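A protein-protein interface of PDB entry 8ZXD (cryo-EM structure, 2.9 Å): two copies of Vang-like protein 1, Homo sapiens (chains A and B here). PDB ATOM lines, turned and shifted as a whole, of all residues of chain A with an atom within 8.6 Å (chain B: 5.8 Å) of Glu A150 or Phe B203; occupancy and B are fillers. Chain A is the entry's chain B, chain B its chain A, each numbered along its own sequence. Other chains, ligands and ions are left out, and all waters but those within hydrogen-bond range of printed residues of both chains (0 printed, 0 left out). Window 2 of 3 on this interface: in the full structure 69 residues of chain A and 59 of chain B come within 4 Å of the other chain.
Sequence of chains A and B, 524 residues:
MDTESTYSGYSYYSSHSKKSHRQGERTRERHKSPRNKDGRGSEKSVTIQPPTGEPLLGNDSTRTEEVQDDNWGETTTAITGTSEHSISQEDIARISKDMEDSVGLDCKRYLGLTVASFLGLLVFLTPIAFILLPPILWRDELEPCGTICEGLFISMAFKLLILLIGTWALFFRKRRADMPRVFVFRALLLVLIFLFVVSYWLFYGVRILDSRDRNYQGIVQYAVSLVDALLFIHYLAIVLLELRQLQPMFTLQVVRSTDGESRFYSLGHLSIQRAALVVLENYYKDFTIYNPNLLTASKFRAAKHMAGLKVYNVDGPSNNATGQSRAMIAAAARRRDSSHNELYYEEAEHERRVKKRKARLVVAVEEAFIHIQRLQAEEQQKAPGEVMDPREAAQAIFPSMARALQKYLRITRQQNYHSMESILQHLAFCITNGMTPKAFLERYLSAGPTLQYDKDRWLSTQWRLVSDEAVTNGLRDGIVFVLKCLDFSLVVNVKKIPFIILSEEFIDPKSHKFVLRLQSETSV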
ATOM      1  N   CYS A 145       3.642 -27.344 -15.150  1.00  0.00           N
ATOM      2  CA  CYS A 145       4.560 -27.934 -16.118  1.00  0.00           C
ATOM      3  C   CYS A 145       5.984 -27.968 -15.579  1.00  0.00           C
ATOM      4  O   CYS A 145       6.687 -28.977 -15.712  1.00  0.00           O
ATOM      5  CB  CYS A 145       4.497 -27.160 -17.435  1.00  0.00           C
ATOM      6  SG  CYS A 145       2.891 -27.221 -18.262  1.00  0.00           S
ATOM      7  N   GLY A 146       6.422 -26.882 -14.970  1.00  0.00           N
ATOM      8  CA  GLY A 146       7.774 -26.803 -14.425  1.00  0.00           C
ATOM      9  C   GLY A 146       8.761 -26.280 -15.462  1.00  0.00           C
ATOM     10  O   GLY A 146       8.617 -25.157 -15.941  1.00  0.00           O
ATOM     11  N   THR A 147       9.757 -27.099 -15.796  1.00  0.00           N
ATOM     12  CA  THR A 147      10.803 -26.708 -16.734  1.00  0.00           C
ATOM     13  C   THR A 147      11.096 -27.755 -17.801  1.00  0.00           C
ATOM     14  O   THR A 147      11.672 -27.402 -18.839  1.00  0.00           O
ATOM     15  CB  THR A 147      12.101 -26.389 -15.973  1.00  0.00           C
ATOM     16  OG1 THR A 147      11.788 -25.593 -14.824  1.00  0.00           O
ATOM     17  CG2 THR A 147      13.073 -25.605 -16.846  1.00  0.00           C
ATOM     18  N   ILE A 148      10.705 -29.016 -17.600  1.00  0.00           N
ATOM     19  CA  ILE A 148      11.007 -30.062 -18.574  1.00  0.00           C
ATOM     20  C   ILE A 148      10.355 -29.754 -19.917  1.00  0.00           C
ATOM     21  O   ILE A 148      10.933 -30.020 -20.979  1.00  0.00           O
ATOM     22  CB  ILE A 148      10.573 -31.438 -18.035  1.00  0.00           C
ATOM     23  CG1 ILE A 148       9.179 -31.354 -17.410  1.00  0.00           C
ATOM     24  CG2 ILE A 148      11.584 -31.956 -17.024  1.00  0.00           C
ATOM     25  CD1 ILE A 148       8.633 -32.689 -16.951  1.00  0.00           C
ATOM     26  N   CYS A 149       9.143 -29.196 -19.894  1.00  0.00           N
ATOM     27  CA  CYS A 149       8.472 -28.836 -21.140  1.00  0.00           C
ATOM     28  C   CYS A 149       9.248 -27.764 -21.896  1.00  0.00           C
ATOM     29  O   CYS A 149       9.392 -27.840 -23.123  1.00  0.00           O
ATOM     30  CB  CYS A 149       7.047 -28.362 -20.852  1.00  0.00           C
ATOM     31  SG  CYS A 149       6.953 -26.752 -20.037  1.00  0.00           S
ATOM     32  N   GLU A 150       9.750 -26.753 -21.182  1.00  0.00           N
ATOM     33  CA  GLU A 150      10.528 -25.703 -21.829  1.00  0.00           C
ATOM     34  C   GLU A 150      11.811 -26.260 -22.434  1.00  0.00           C
ATOM     35  O   GLU A 150      12.198 -25.880 -23.546  1.00  0.00           O
ATOM     36  CB  GLU A 150      10.845 -24.591 -20.829  1.00  0.00           C
ATOM     37  CG  GLU A 150      11.374 -23.316 -21.463  1.00  0.00           C
ATOM     38  CD  GLU A 150      10.301 -22.544 -22.205  1.00  0.00           C
ATOM     39  OE1 GLU A 150       9.114 -22.670 -21.836  1.00  0.00           O
ATOM     40  OE2 GLU A 150      10.644 -21.812 -23.157  1.00  0.00           O
ATOM     41  N   GLY A 151      12.486 -27.159 -21.715  1.00  0.00           N
ATOM     42  CA  GLY A 151      13.688 -27.773 -22.252  1.00  0.00           C
ATOM     43  C   GLY A 151      13.422 -28.660 -23.449  1.00  0.00           C
ATOM     44  O   GLY A 151      14.245 -28.734 -24.365  1.00  0.00           O
ATOM     45  N   LEU A 152      12.281 -29.352 -23.460  1.00  0.00           N
ATOM     46  CA  LEU A 152      11.948 -30.219 -24.583  1.00  0.00           C
ATOM     47  C   LEU A 152      11.472 -29.433 -25.799  1.00  0.00           C
ATOM     48  O   LEU A 152      11.643 -29.897 -26.932  1.00  0.00           O
ATOM     49  CB  LEU A 152      10.882 -31.235 -24.166  1.00  0.00           C
ATOM     50  CG  LEU A 152      11.364 -32.397 -23.295  1.00  0.00           C
ATOM     51  CD1 LEU A 152      10.239 -33.394 -23.056  1.00  0.00           C
ATOM     52  CD2 LEU A 152      12.566 -33.082 -23.926  1.00  0.00           C
ATOM     53  N   PHE A 153      10.875 -28.258 -25.589  1.00  0.00           N
ATOM     54  CA  PHE A 153      10.353 -27.478 -26.708  1.00  0.00           C
ATOM     55  C   PHE A 153      11.468 -27.049 -27.656  1.00  0.00           C
ATOM     56  O   PHE A 153      11.337 -27.162 -28.881  1.00  0.00           O
ATOM     57  CB  PHE A 153       9.597 -26.256 -26.183  1.00  0.00           C
ATOM     58  CG  PHE A 153       8.195 -26.555 -25.735  1.00  0.00           C
ATOM     59  CD1 PHE A 153       7.532 -27.680 -26.195  1.00  0.00           C
ATOM     60  CD2 PHE A 153       7.541 -25.712 -24.852  1.00  0.00           C
ATOM     61  CE1 PHE A 153       6.241 -27.958 -25.784  1.00  0.00           C
ATOM     62  CE2 PHE A 153       6.251 -25.985 -24.438  1.00  0.00           C
ATOM     63  CZ  PHE A 153       5.601 -27.109 -24.904  1.00  0.00           C
ATOM     64  N   ILE A 154      12.579 -26.556 -27.105  1.00  0.00           N
ATOM     65  CA  ILE A 154      13.670 -26.078 -27.949  1.00  0.00           C
ATOM     66  C   ILE A 154      14.346 -27.242 -28.665  1.00  0.00           C
ATOM     67  O   ILE A 154      14.739 -27.126 -29.833  1.00  0.00           O
ATOM     68  CB  ILE A 154      14.669 -25.255 -27.114  1.00  0.00           C
ATOM     69  CG1 ILE A 154      15.890 -24.883 -27.952  1.00  0.00           C
ATOM     70  CG2 ILE A 154      15.086 -26.010 -25.861  1.00  0.00           C
ATOM     71  CD1 ILE A 154      16.830 -23.952 -27.248  1.00  0.00           C
ATOM     72  N   SER A 155      14.490 -28.381 -27.983  1.00  0.00           N
ATOM     73  CA  SER A 155      15.049 -29.563 -28.632  1.00  0.00           C
ATOM     74  C   SER A 155      14.157 -30.032 -29.774  1.00  0.00           C
ATOM     75  O   SER A 155      14.652 -30.407 -30.845  1.00  0.00           O
ATOM     76  CB  SER A 155      15.247 -30.679 -27.608  1.00  0.00           C
ATOM     77  OG  SER A 155      14.003 -31.156 -27.125  1.00  0.00           O
ATOM     78  N   MET A 156      12.838 -30.012 -29.568  1.00  0.00           N
ATOM     79  CA  MET A 156      11.914 -30.385 -30.632  1.00  0.00           C
ATOM     80  C   MET A 156      12.005 -29.418 -31.805  1.00  0.00           C
ATOM     81  O   MET A 156      11.962 -29.834 -32.968  1.00  0.00           O
ATOM     82  CB  MET A 156      10.486 -30.439 -30.088  1.00  0.00           C
ATOM     83  CG  MET A 156       9.546 -31.319 -30.891  1.00  0.00           C
ATOM     84  SD  MET A 156       7.814 -31.001 -30.506  1.00  0.00           S
ATOM     85  CE  MET A 156       7.637 -29.325 -31.109  1.00  0.00           C
ATOM     86  N   ALA A 157      12.126 -28.118 -31.519  1.00  0.00           N
ATOM     87  CA  ALA A 157      12.266 -27.136 -32.591  1.00  0.00           C
ATOM     88  C   ALA A 157      13.548 -27.359 -33.384  1.00  0.00           C
ATOM     89  O   ALA A 157      13.548 -27.280 -34.619  1.00  0.00           O
ATOM     90  CB  ALA A 157      12.227 -25.721 -32.015  1.00  0.00           C
ATOM     91  N   TYR A 216      -0.080 -32.029 -19.334  1.00  0.00           N
ATOM     92  CA  TYR A 216       0.817 -31.489 -20.352  1.00  0.00           C
ATOM     93  C   TYR A 216       2.214 -32.090 -20.247  1.00  0.00           C
ATOM     94  O   TYR A 216       2.844 -32.391 -21.268  1.00  0.00           O
ATOM     95  CB  TYR A 216       0.880 -29.966 -20.236  1.00  0.00           C
ATOM     96  CG  TYR A 216       1.296 -29.270 -21.512  1.00  0.00           C
ATOM     97  CD1 TYR A 216       0.404 -29.119 -22.566  1.00  0.00           C
ATOM     98  CD2 TYR A 216       2.579 -28.762 -21.663  1.00  0.00           C
ATOM     99  CE1 TYR A 216       0.779 -28.484 -23.734  1.00  0.00           C
ATOM    100  CE2 TYR A 216       2.963 -28.124 -22.827  1.00  0.00           C
ATOM    101  CZ  TYR A 216       2.059 -27.989 -23.860  1.00  0.00           C
ATOM    102  OH  TYR A 216       2.436 -27.355 -25.022  1.00  0.00           O
ATOM    103  N   VAL A 220       4.504 -33.673 -23.809  1.00  0.00           N
ATOM    104  CA  VAL A 220       5.699 -33.149 -24.466  1.00  0.00           C
ATOM    105  C   VAL A 220       6.712 -34.263 -24.711  1.00  0.00           C
ATOM    106  O   VAL A 220       7.306 -34.353 -25.793  1.00  0.00           O
ATOM    107  CB  VAL A 220       6.297 -31.984 -23.652  1.00  0.00           C
ATOM    108  CG1 VAL A 220       5.300 -30.841 -23.570  1.00  0.00           C
ATOM    109  CG2 VAL A 220       6.682 -32.431 -22.249  1.00  0.00           C
ATOM    110  N   VAL B 198      25.025 -22.186 -27.569  1.00  0.00           N
ATOM    111  CA  VAL B 198      24.852 -20.984 -26.756  1.00  0.00           C
ATOM    112  C   VAL B 198      23.437 -20.901 -26.192  1.00  0.00           C
ATOM    113  O   VAL B 198      23.238 -20.431 -25.067  1.00  0.00           O
ATOM    114  CB  VAL B 198      25.224 -19.716 -27.551  1.00  0.00           C
ATOM    115  CG1 VAL B 198      26.681 -19.766 -27.994  1.00  0.00           C
ATOM    116  CG2 VAL B 198      24.293 -19.508 -28.737  1.00  0.00           C
ATOM    117  N   SER B 199      22.429 -21.333 -26.957  1.00  0.00           N
ATOM    118  CA  SER B 199      21.062 -21.257 -26.456  1.00  0.00           C
ATOM    119  C   SER B 199      20.869 -22.176 -25.256  1.00  0.00           C
ATOM    120  O   SER B 199      20.250 -21.786 -24.257  1.00  0.00           O
ATOM    121  CB  SER B 199      20.073 -21.594 -27.569  1.00  0.00           C
ATOM    122  OG  SER B 199      18.745 -21.551 -27.084  1.00  0.00           O
ATOM    123  N   TYR B 200      21.405 -23.399 -25.328  1.00  0.00           N
ATOM    124  CA  TYR B 200      21.335 -24.299 -24.181  1.00  0.00           C
ATOM    125  C   TYR B 200      22.127 -23.754 -23.002  1.00  0.00           C
ATOM    126  O   TYR B 200      21.704 -23.895 -21.849  1.00  0.00           O
ATOM    127  CB  TYR B 200      21.835 -25.697 -24.549  1.00  0.00           C
ATOM    128  CG  TYR B 200      20.948 -26.453 -25.509  1.00  0.00           C
ATOM    129  CD1 TYR B 200      19.651 -26.032 -25.768  1.00  0.00           C
ATOM    130  CD2 TYR B 200      21.392 -27.615 -26.119  1.00  0.00           C
ATOM    131  CE1 TYR B 200      18.835 -26.732 -26.637  1.00  0.00           C
ATOM    132  CE2 TYR B 200      20.580 -28.322 -26.980  1.00  0.00           C
ATOM    133  CZ  TYR B 200      19.305 -27.876 -27.240  1.00  0.00           C
ATOM    134  OH  TYR B 200      18.491 -28.577 -28.103  1.00  0.00           O
ATOM    135  N   TRP B 201      23.290 -23.151 -23.260  1.00  0.00           N
ATOM    136  CA  TRP B 201      24.066 -22.581 -22.161  1.00  0.00           C
ATOM    137  C   TRP B 201      23.297 -21.464 -21.464  1.00  0.00           C
ATOM    138  O   TRP B 201      23.257 -21.406 -20.229  1.00  0.00           O
ATOM    139  CB  TRP B 201      25.413 -22.073 -22.672  1.00  0.00           C
ATOM    140  CG  TRP B 201      26.508 -23.078 -22.530  1.00  0.00           C
ATOM    141  CD1 TRP B 201      27.121 -23.770 -23.531  1.00  0.00           C
ATOM    142  CD2 TRP B 201      27.111 -23.521 -21.308  1.00  0.00           C
ATOM    143  NE1 TRP B 201      28.076 -24.609 -23.010  1.00  0.00           N
ATOM    144  CE2 TRP B 201      28.089 -24.475 -21.646  1.00  0.00           C
ATOM    145  CE3 TRP B 201      26.921 -23.198 -19.960  1.00  0.00           C
ATOM    146  CZ2 TRP B 201      28.875 -25.112 -20.688  1.00  0.00           C
ATOM    147  CZ3 TRP B 201      27.702 -23.830 -19.010  1.00  0.00           C
ATOM    148  CH2 TRP B 201      28.667 -24.776 -19.379  1.00  0.00           C
ATOM    149  N   LEU B 202      22.669 -20.578 -22.240  1.00  0.00           N
ATOM    150  CA  LEU B 202      21.879 -19.503 -21.650  1.00  0.00           C
ATOM    151  C   LEU B 202      20.683 -20.055 -20.884  1.00  0.00           C
ATOM    152  O   LEU B 202      20.359 -19.571 -19.793  1.00  0.00           O
ATOM    153  CB  LEU B 202      21.416 -18.530 -22.734  1.00  0.00           C
ATOM    154  CG  LEU B 202      22.453 -17.556 -23.299  1.00  0.00           C
ATOM    155  CD1 LEU B 202      21.868 -16.783 -24.470  1.00  0.00           C
ATOM    156  CD2 LEU B 202      22.952 -16.605 -22.220  1.00  0.00           C
ATOM    157  N   PHE B 203      20.014 -21.069 -21.440  1.00  0.00           N
ATOM    158  CA  PHE B 203      18.881 -21.675 -20.749  1.00  0.00           C
ATOM    159  C   PHE B 203      19.309 -22.291 -19.423  1.00  0.00           C
ATOM    160  O   PHE B 203      18.635 -22.116 -18.401  1.00  0.00           O
ATOM    161  CB  PHE B 203      18.226 -22.725 -21.647  1.00  0.00           C
ATOM    162  CG  PHE B 203      17.074 -23.443 -21.004  1.00  0.00           C
ATOM    163  CD1 PHE B 203      15.867 -22.798 -20.795  1.00  0.00           C
ATOM    164  CD2 PHE B 203      17.198 -24.766 -20.615  1.00  0.00           C
ATOM    165  CE1 PHE B 203      14.806 -23.457 -20.205  1.00  0.00           C
ATOM    166  CE2 PHE B 203      16.140 -25.432 -20.024  1.00  0.00           C
ATOM    167  CZ  PHE B 203      14.942 -24.776 -19.820  1.00  0.00           C
ATOM    168  N   TYR B 204      20.436 -23.008 -19.419  1.00  0.00           N
ATOM    169  CA  TYR B 204      20.934 -23.612 -18.188  1.00  0.00           C
ATOM    170  C   TYR B 204      21.321 -22.548 -17.169  1.00  0.00           C
ATOM    171  O   TYR B 204      21.059 -22.703 -15.970  1.00  0.00           O
ATOM    172  CB  TYR B 204      22.125 -24.520 -18.498  1.00  0.00           C
ATOM    173  CG  TYR B 204      22.479 -25.476 -17.380  1.00  0.00           C
ATOM    174  CD1 TYR B 204      21.853 -26.712 -17.276  1.00  0.00           C
ATOM    175  CD2 TYR B 204      23.435 -25.143 -16.431  1.00  0.00           C
ATOM    176  CE1 TYR B 204      22.172 -27.590 -16.257  1.00  0.00           C
ATOM    177  CE2 TYR B 204      23.759 -26.015 -15.408  1.00  0.00           C
ATOM    178  CZ  TYR B 204      23.126 -27.236 -15.326  1.00  0.00           C
ATOM    179  OH  TYR B 204      23.447 -28.105 -14.309  1.00  0.00           O
ATOM    180  N   GLY B 205      21.948 -21.462 -17.624  1.00  0.00           N
ATOM    181  CA  GLY B 205      22.375 -20.419 -16.709  1.00  0.00           C
ATOM    182  C   GLY B 205      21.254 -19.544 -16.186  1.00  0.00           C
ATOM    183  O   GLY B 205      21.409 -18.930 -15.126  1.00  0.00           O
ATOM    184  N   VAL B 206      20.134 -19.473 -16.899  1.00  0.00           N
ATOM    185  CA  VAL B 206      19.030 -18.595 -16.524  1.00  0.00           C
ATOM    186  C   VAL B 206      17.929 -19.351 -15.789  1.00  0.00           C
ATOM    187  O   VAL B 206      17.544 -18.977 -14.680  1.00  0.00           O
ATOM    188  CB  VAL B 206      18.476 -17.873 -17.773  1.00  0.00           C
ATOM    189  CG1 VAL B 206      17.100 -17.289 -17.487  1.00  0.00           C
ATOM    190  CG2 VAL B 206      19.439 -16.789 -18.229  1.00  0.00           C
ATOM    191  N   ARG B 207      17.406 -20.420 -16.388  1.00  0.00           N
ATOM    192  CA  ARG B 207      16.229 -21.093 -15.855  1.00  0.00           C
ATOM    193  C   ARG B 207      16.547 -22.129 -14.785  1.00  0.00           C
ATOM    194  O   ARG B 207      15.615 -22.703 -14.210  1.00  0.00           O
ATOM    195  CB  ARG B 207      15.449 -21.764 -16.991  1.00  0.00           C
ATOM    196  CG  ARG B 207      14.627 -20.800 -17.833  1.00  0.00           C
ATOM    197  CD  ARG B 207      13.359 -20.376 -17.110  1.00  0.00           C
ATOM    198  NE  ARG B 207      12.379 -19.799 -18.023  1.00  0.00           N
ATOM    199  CZ  ARG B 207      11.182 -19.361 -17.658  1.00  0.00           C
ATOM    200  NH1 ARG B 207      10.778 -19.421 -16.401  1.00  0.00           N
ATOM    201  NH2 ARG B 207      10.370 -18.851 -18.579  1.00  0.00           N
ATOM    202  N   ILE B 208      17.820 -22.388 -14.501  1.00  0.00           N
ATOM    203  CA  ILE B 208      18.223 -23.409 -13.541  1.00  0.00           C
ATOM    204  C   ILE B 208      19.068 -22.819 -12.417  1.00  0.00           C
ATOM    205  O   ILE B 208      18.763 -23.003 -11.237  1.00  0.00           O
ATOM    206  CB  ILE B 208      18.967 -24.566 -14.245  1.00  0.00           C
ATOM    207  CG1 ILE B 208      18.031 -25.284 -15.221  1.00  0.00           C
ATOM    208  CG2 ILE B 208      19.528 -25.540 -13.220  1.00  0.00           C
ATOM    209  CD1 ILE B 208      18.610 -26.551 -15.809  1.00  0.00           C
ATOM    210  N   TYR B 222      17.076 -33.958 -19.529  1.00  0.00           N
ATOM    211  CA  TYR B 222      17.517 -32.843 -20.359  1.00  0.00           C
ATOM    212  C   TYR B 222      18.888 -33.119 -20.963  1.00  0.00           C
ATOM    213  O   TYR B 222      19.126 -32.824 -22.141  1.00  0.00           O
ATOM    214  CB  TYR B 222      17.537 -31.556 -19.537  1.00  0.00           C
ATOM    215  CG  TYR B 222      17.914 -30.323 -20.326  1.00  0.00           C
ATOM    216  CD1 TYR B 222      17.020 -29.746 -21.219  1.00  0.00           C
ATOM    217  CD2 TYR B 222      19.163 -29.735 -20.178  1.00  0.00           C
ATOM    218  CE1 TYR B 222      17.360 -28.617 -21.942  1.00  0.00           C
ATOM    219  CE2 TYR B 222      19.513 -28.607 -20.896  1.00  0.00           C
ATOM    220  CZ  TYR B 222      18.608 -28.053 -21.777  1.00  0.00           C
ATOM    221  OH  TYR B 222      18.951 -26.930 -22.495  1.00  0.00           O
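Of the 15 printed residues of chain A, 5 touch a printed residue of chain B. Printed residues of chain A that touch a printed residue of chain B: Thr A147, Glu A150, Gly A151, Ile A154 and Ser A155. Hydrophobic or aromatic side chains of chain A that line the printed part of chain B: Ile A154. Along chain A the printed residues that touch a printed residue of chain B span positions 147 to 155. Hydrophobic or aromatic side chains of chain B within 4 Å of the printed part of chain A: Tyr B200, Phe B203 and Tyr B222. Along chain B the printed residues that touch a printed residue of chain A span positions 199 to 222. Among the printed residues, no Asp or Glu carboxylate lies within 4 Å of a Lys or Arg side-chain nitrogen of the other chain.
Printed residues of chain B within 4 Å of Thr A147: Phe B203 (3.6 Å). Printed residues of chain B within 4 Å of Glu A150: Phe B203 (3.7 Å). Printed residues of chain A within 4 Å of Ser B199: Ile A154 (3.1 Å). Of the printed residues of chain A, Tyr B200 touches Ile A154 (3.5 Å) and Ser A155 (3.6 Å). Of chain A, only Thr A147, Glu A150 and Gly A151 come within 4 Å of Phe B203. The nearest residue of chain A that does not touch Phe B203 is Ile A154 (5.8 Å). The nearest printed residue of chain A that does not touch Ser B199 is Ser A155 (8.1 Å).
OG of Ser A155 sits at hydrogen-bond distance from O of Leu A152 (2.7 Å).
No position is printed for both chains. Of the 7 pairs that touch across the chains among the printed residues, none has its exchanged pair printed and touching as well.
Among the printed residues, pairs that only touch across the chains: Ile A154 with Ser B199, Ile A154 with Tyr B200, Thr A147 with Phe B203, Ser A155 with Tyr B200, Glu A150 with Phe B203, Gly A151 with Tyr B222 and Gly A151 with Phe B203.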
